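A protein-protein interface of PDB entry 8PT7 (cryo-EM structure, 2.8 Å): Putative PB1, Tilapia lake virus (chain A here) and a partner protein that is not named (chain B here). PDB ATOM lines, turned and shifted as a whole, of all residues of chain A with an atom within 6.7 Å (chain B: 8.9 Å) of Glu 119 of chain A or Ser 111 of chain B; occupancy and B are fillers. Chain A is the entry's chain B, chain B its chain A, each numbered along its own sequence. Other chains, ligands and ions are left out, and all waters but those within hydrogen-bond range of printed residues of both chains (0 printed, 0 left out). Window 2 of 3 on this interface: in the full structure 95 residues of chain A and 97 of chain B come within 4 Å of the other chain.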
ATOM      1  N   LEU A 116     -28.955 -11.845 -11.199  1.00  0.00           N
ATOM      2  CA  LEU A 116     -27.550 -12.113 -10.927  1.00  0.00           C
ATOM      3  C   LEU A 116     -27.247 -12.288  -9.445  1.00  0.00           C
ATOM      4  O   LEU A 116     -26.123 -12.674  -9.108  1.00  0.00           O
ATOM      5  CB  LEU A 116     -26.684 -10.985 -11.492  1.00  0.00           C
ATOM      6  CG  LEU A 116     -26.302 -11.111 -12.968  1.00  0.00           C
ATOM      7  CD1 LEU A 116     -25.640  -9.834 -13.450  1.00  0.00           C
ATOM      8  CD2 LEU A 116     -25.387 -12.304 -13.193  1.00  0.00           C
ATOM      9  N   THR A 117     -28.203 -12.021  -8.557  1.00  0.00           N
ATOM     10  CA  THR A 117     -27.966 -12.032  -7.114  1.00  0.00           C
ATOM     11  C   THR A 117     -29.009 -12.882  -6.396  1.00  0.00           C
ATOM     12  O   THR A 117     -29.620 -12.459  -5.414  1.00  0.00           O
ATOM     13  CB  THR A 117     -27.963 -10.614  -6.551  1.00  0.00           C
ATOM     14  OG1 THR A 117     -29.282 -10.058  -6.637  1.00  0.00           O
ATOM     15  CG2 THR A 117     -26.990  -9.731  -7.318  1.00  0.00           C
ATOM     16  N   VAL A 118     -29.226 -14.102  -6.881  1.00  0.00           N
ATOM     17  CA  VAL A 118     -30.084 -15.069  -6.207  1.00  0.00           C
ATOM     18  C   VAL A 118     -29.212 -16.186  -5.658  1.00  0.00           C
ATOM     19  O   VAL A 118     -28.124 -16.468  -6.174  1.00  0.00           O
ATOM     20  CB  VAL A 118     -31.180 -15.643  -7.130  1.00  0.00           C
ATOM     21  CG1 VAL A 118     -32.279 -14.619  -7.347  1.00  0.00           C
ATOM     22  CG2 VAL A 118     -30.587 -16.093  -8.451  1.00  0.00           C
ATOM     23  N   GLU A 119     -29.698 -16.828  -4.594  1.00  0.00           N
ATOM     24  CA  GLU A 119     -28.914 -17.871  -3.941  1.00  0.00           C
ATOM     25  C   GLU A 119     -28.913 -19.166  -4.742  1.00  0.00           C
ATOM     26  O   GLU A 119     -27.900 -19.874  -4.765  1.00  0.00           O
ATOM     27  CB  GLU A 119     -29.448 -18.128  -2.530  1.00  0.00           C
ATOM     28  CG  GLU A 119     -29.795 -16.872  -1.732  1.00  0.00           C
ATOM     29  CD  GLU A 119     -28.582 -16.021  -1.397  1.00  0.00           C
ATOM     30  OE1 GLU A 119     -27.595 -16.048  -2.161  1.00  0.00           O
ATOM     31  OE2 GLU A 119     -28.617 -15.320  -0.364  1.00  0.00           O
ATOM     32  N   SER A 120     -30.021 -19.492  -5.403  1.00  0.00           N
ATOM     33  CA  SER A 120     -30.121 -20.742  -6.142  1.00  0.00           C
ATOM     34  C   SER A 120     -31.009 -20.540  -7.359  1.00  0.00           C
ATOM     35  O   SER A 120     -31.789 -19.587  -7.435  1.00  0.00           O
ATOM     36  CB  SER A 120     -30.671 -21.871  -5.262  1.00  0.00           C
ATOM     37  OG  SER A 120     -32.002 -21.598  -4.859  1.00  0.00           O
ATOM     38  N   LEU A 121     -30.876 -21.457  -8.319  1.00  0.00           N
ATOM     39  CA  LEU A 121     -31.702 -21.395  -9.519  1.00  0.00           C
ATOM     40  C   LEU A 121     -33.179 -21.552  -9.186  1.00  0.00           C
ATOM     41  O   LEU A 121     -34.035 -21.002  -9.888  1.00  0.00           O
ATOM     42  CB  LEU A 121     -31.266 -22.474 -10.510  1.00  0.00           C
ATOM     43  CG  LEU A 121     -29.935 -22.238 -11.222  1.00  0.00           C
ATOM     44  CD1 LEU A 121     -29.473 -23.508 -11.916  1.00  0.00           C
ATOM     45  CD2 LEU A 121     -30.051 -21.097 -12.217  1.00  0.00           C
ATOM     46  N   SER A 122     -33.497 -22.298  -8.129  1.00  0.00           N
ATOM     47  CA  SER A 122     -34.884 -22.524  -7.743  1.00  0.00           C
ATOM     48  C   SER A 122     -35.483 -21.364  -6.960  1.00  0.00           C
ATOM     49  O   SER A 122     -36.695 -21.361  -6.725  1.00  0.00           O
ATOM     50  CB  SER A 122     -34.991 -23.804  -6.912  1.00  0.00           C
ATOM     51  OG  SER A 122     -34.111 -23.765  -5.803  1.00  0.00           O
ATOM     52  N   GLU A 123     -34.675 -20.387  -6.553  1.00  0.00           N
ATOM     53  CA  GLU A 123     -35.207 -19.245  -5.824  1.00  0.00           C
ATOM     54  C   GLU A 123     -36.183 -18.469  -6.699  1.00  0.00           C
ATOM     55  O   GLU A 123     -36.017 -18.366  -7.917  1.00  0.00           O
ATOM     56  CB  GLU A 123     -34.071 -18.330  -5.365  1.00  0.00           C
ATOM     57  CG  GLU A 123     -34.547 -17.034  -4.728  1.00  0.00           C
ATOM     58  CD  GLU A 123     -33.507 -16.412  -3.816  1.00  0.00           C
ATOM     59  OE1 GLU A 123     -32.803 -17.164  -3.110  1.00  0.00           O
ATOM     60  OE2 GLU A 123     -33.398 -15.169  -3.801  1.00  0.00           O
ATOM     61  N   SER A 237     -21.300 -14.469 -15.242  1.00  0.00           N
ATOM     62  CA  SER A 237     -22.374 -15.451 -15.337  1.00  0.00           C
ATOM     63  C   SER A 237     -23.344 -15.161 -16.475  1.00  0.00           C
ATOM     64  O   SER A 237     -24.067 -16.069 -16.895  1.00  0.00           O
ATOM     65  CB  SER A 237     -23.137 -15.517 -14.015  1.00  0.00           C
ATOM     66  OG  SER A 237     -22.373 -16.178 -13.023  1.00  0.00           O
ATOM     67  N   HIS B 108     -19.773 -10.066 -12.867  1.00  0.00           N
ATOM     68  CA  HIS B 108     -20.237 -10.622 -11.603  1.00  0.00           C
ATOM     69  C   HIS B 108     -20.462 -12.122 -11.734  1.00  0.00           C
ATOM     70  O   HIS B 108     -21.056 -12.592 -12.707  1.00  0.00           O
ATOM     71  CB  HIS B 108     -21.528  -9.929 -11.172  1.00  0.00           C
ATOM     72  CG  HIS B 108     -22.110 -10.471  -9.903  1.00  0.00           C
ATOM     73  ND1 HIS B 108     -22.899 -11.599  -9.869  1.00  0.00           N
ATOM     74  CD2 HIS B 108     -22.021 -10.035  -8.624  1.00  0.00           C
ATOM     75  CE1 HIS B 108     -23.267 -11.838  -8.623  1.00  0.00           C
ATOM     76  NE2 HIS B 108     -22.749 -10.902  -7.849  1.00  0.00           N
ATOM     77  N   LYS B 109     -19.984 -12.873 -10.743  1.00  0.00           N
ATOM     78  CA  LYS B 109     -20.114 -14.327 -10.730  1.00  0.00           C
ATOM     79  C   LYS B 109     -21.271 -14.706  -9.813  1.00  0.00           C
ATOM     80  O   LYS B 109     -21.222 -14.459  -8.605  1.00  0.00           O
ATOM     81  CB  LYS B 109     -18.812 -14.977 -10.268  1.00  0.00           C
ATOM     82  CG  LYS B 109     -18.644 -16.418 -10.739  1.00  0.00           C
ATOM     83  CD  LYS B 109     -17.335 -17.050 -10.270  1.00  0.00           C
ATOM     84  CE  LYS B 109     -17.069 -16.838  -8.785  1.00  0.00           C
ATOM     85  NZ  LYS B 109     -18.233 -17.233  -7.942  1.00  0.00           N
ATOM     86  N   ALA B 110     -22.308 -15.308 -10.387  1.00  0.00           N
ATOM     87  CA  ALA B 110     -23.463 -15.723  -9.611  1.00  0.00           C
ATOM     88  C   ALA B 110     -23.172 -17.026  -8.872  1.00  0.00           C
ATOM     89  O   ALA B 110     -22.210 -17.740  -9.167  1.00  0.00           O
ATOM     90  CB  ALA B 110     -24.683 -15.894 -10.513  1.00  0.00           C
ATOM     91  N   SER B 111     -24.026 -17.329  -7.894  1.00  0.00           N
ATOM     92  CA  SER B 111     -23.857 -18.537  -7.095  1.00  0.00           C
ATOM     93  C   SER B 111     -24.154 -19.809  -7.875  1.00  0.00           C
ATOM     94  O   SER B 111     -23.811 -20.896  -7.401  1.00  0.00           O
ATOM     95  CB  SER B 111     -24.756 -18.472  -5.861  1.00  0.00           C
ATOM     96  OG  SER B 111     -26.104 -18.735  -6.203  1.00  0.00           O
ATOM     97  N   TYR B 112     -24.777 -19.704  -9.048  1.00  0.00           N
ATOM     98  CA  TYR B 112     -25.099 -20.861  -9.873  1.00  0.00           C
ATOM     99  C   TYR B 112     -24.148 -21.017 -11.052  1.00  0.00           C
ATOM    100  O   TYR B 112     -24.418 -21.817 -11.952  1.00  0.00           O
ATOM    101  CB  TYR B 112     -26.542 -20.769 -10.379  1.00  0.00           C
ATOM    102  CG  TYR B 112     -26.956 -19.387 -10.828  1.00  0.00           C
ATOM    103  CD1 TYR B 112     -26.682 -18.944 -12.114  1.00  0.00           C
ATOM    104  CD2 TYR B 112     -27.619 -18.526  -9.966  1.00  0.00           C
ATOM    105  CE1 TYR B 112     -27.056 -17.683 -12.528  1.00  0.00           C
ATOM    106  CE2 TYR B 112     -27.998 -17.263 -10.374  1.00  0.00           C
ATOM    107  CZ  TYR B 112     -27.714 -16.846 -11.654  1.00  0.00           C
ATOM    108  OH  TYR B 112     -28.091 -15.588 -12.060  1.00  0.00           O
ATOM    109  N   ASP B 113     -23.040 -20.272 -11.068  1.00  0.00           N
ATOM    110  CA  ASP B 113     -22.115 -20.350 -12.194  1.00  0.00           C
ATOM    111  C   ASP B 113     -21.546 -21.754 -12.346  1.00  0.00           C
ATOM    112  O   ASP B 113     -21.488 -22.290 -13.459  1.00  0.00           O
ATOM    113  CB  ASP B 113     -20.987 -19.336 -12.008  1.00  0.00           C
ATOM    114  CG  ASP B 113     -20.413 -18.855 -13.324  1.00  0.00           C
ATOM    115  OD1 ASP B 113     -19.609 -19.595 -13.928  1.00  0.00           O
ATOM    116  OD2 ASP B 113     -20.765 -17.738 -13.755  1.00  0.00           O
ATOM    117  N   ALA B 114     -21.125 -22.368 -11.239  1.00  0.00           N
ATOM    118  CA  ALA B 114     -20.530 -23.698 -11.316  1.00  0.00           C
ATOM    119  C   ALA B 114     -21.532 -24.724 -11.827  1.00  0.00           C
ATOM    120  O   ALA B 114     -21.192 -25.573 -12.660  1.00  0.00           O
ATOM    121  CB  ALA B 114     -19.994 -24.111  -9.945  1.00  0.00           C
ATOM    122  N   GLU B 115     -22.771 -24.667 -11.337  1.00  0.00           N
ATOM    123  CA  GLU B 115     -23.780 -25.630 -11.766  1.00  0.00           C
ATOM    124  C   GLU B 115     -24.068 -25.494 -13.255  1.00  0.00           C
ATOM    125  O   GLU B 115     -24.154 -26.495 -13.979  1.00  0.00           O
ATOM    126  CB  GLU B 115     -25.058 -25.439 -10.949  1.00  0.00           C
ATOM    127  CG  GLU B 115     -26.110 -26.508 -11.183  1.00  0.00           C
ATOM    128  CD  GLU B 115     -27.385 -26.244 -10.409  1.00  0.00           C
ATOM    129  OE1 GLU B 115     -27.506 -25.150  -9.820  1.00  0.00           O
ATOM    130  OE2 GLU B 115     -28.265 -27.129 -10.388  1.00  0.00           O
ATOM    131  N   LEU B 116     -24.223 -24.258 -13.734  1.00  0.00           N
ATOM    132  CA  LEU B 116     -24.498 -24.048 -15.150  1.00  0.00           C
ATOM    133  C   LEU B 116     -23.318 -24.486 -16.008  1.00  0.00           C
ATOM    134  O   LEU B 116     -23.506 -25.064 -17.085  1.00  0.00           O
ATOM    135  CB  LEU B 116     -24.833 -22.579 -15.408  1.00  0.00           C
ATOM    136  CG  LEU B 116     -26.209 -22.095 -14.938  1.00  0.00           C
ATOM    137  CD1 LEU B 116     -26.434 -20.659 -15.373  1.00  0.00           C
ATOM    138  CD2 LEU B 116     -27.324 -22.989 -15.461  1.00  0.00           C
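Among the printed residues, pairs that only touch across the chains: Leu 116 of chain A with Ala 110 of chain B (3.8 Å), Leu 116 of chain A with Tyr 112 of chain B (3.7 Å), Val 118 of chain A with Tyr 112 of chain B (3.4 Å), Leu 121 of chain A with Tyr 112 of chain B (3.8 Å), Leu 121 of chain A with Glu 115 of chain B (3.3 Å) and Ser 237 of chain A with Lys 109 of chain B (3.7 Å).
Printed residues of chain B that touch a printed residue of chain A: His 108, Lys 109, Ala 110, Ser 111, Tyr 112, Asp 113 and Glu 115. Hydrophobic or aromatic side chains of chain B that line the printed part of chain A: His 108, Ala 110 and Tyr 112. Printed residues of chain A that touch a printed residue of chain B: Leu 116, Val 118, Glu 119, Leu 121 and Ser 237. Hydrophobic or aromatic side chains of chain A within 4 Å of the printed part of chain B: Val 118 and Leu 121.
The backbone NH (N) of Ala 110 of chain B is in hydrogen-bond range of the side-chain hydroxyl (OG) of Ser 237 of chain A (2.8 Å). N of Ser 237 of chain A is in hydrogen-bond range of O of His 108 of chain B. The side-chain hydroxyl of Ser 111 of chain B lies within hydrogen-bond range of the backbone carbonyl oxygen of Val 118 of chain A, 3.0 Å away. The side-chain hydroxyl (OG) of Ser 111 of chain B lies within hydrogen-bond range of the backbone carbonyl oxygen (O) of Glu 119 of chain A. The backbone carbonyl oxygen (O) of Leu 116 of chain A lies close to a ring nitrogen (ND1) of His 108 of chain B. The side-chain carboxylate (OD2) of Asp 113 of chain B lies close to the side-chain hydroxyl (OG) of Ser 237 of chain A.
The side-chain carboxylate of Glu 123 of chain A lies close to the backbone NH of Glu 119 of chain A.
Glu 119 of chain A touches just one residue of chain B: Ser 111. Ser 111 of chain B touches just these residues of chain A: Val 118 and Glu 119. Val 118 of chain A touches just these residues of chain B: Ser 111 (3.0 Å) and Tyr 112 (3.4 Å). No residue of chain B comes within 4 Å of Ser 120 of chain A. Printed residues of chain A within 4 Å of Ala 110 of chain B: Leu 116 (3.8 Å) and Ser 237 (2.8 Å). Of the printed residues of chain B, Leu 116 of chain A touches His 108 (3.0 Å), Ala 110 (3.8 Å) and Tyr 112 (3.7 Å). Of the printed residues of chain A, Lys 109 of chain B touches Ser 237. Printed residues of chain A within 4 Å of Tyr 112 of chain B: Leu 116 (3.7 Å), Val 118 (3.4 Å) and Leu 121 (3.8 Å). Thr 117 of chain A touches none of the printed residues of chain B. Ser 122 of chain A touches none of the printed residues of chain B. The nearest printed residue of chain A that does not touch Asp 113 of chain B is Leu 121 of chain A (7.2 Å).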
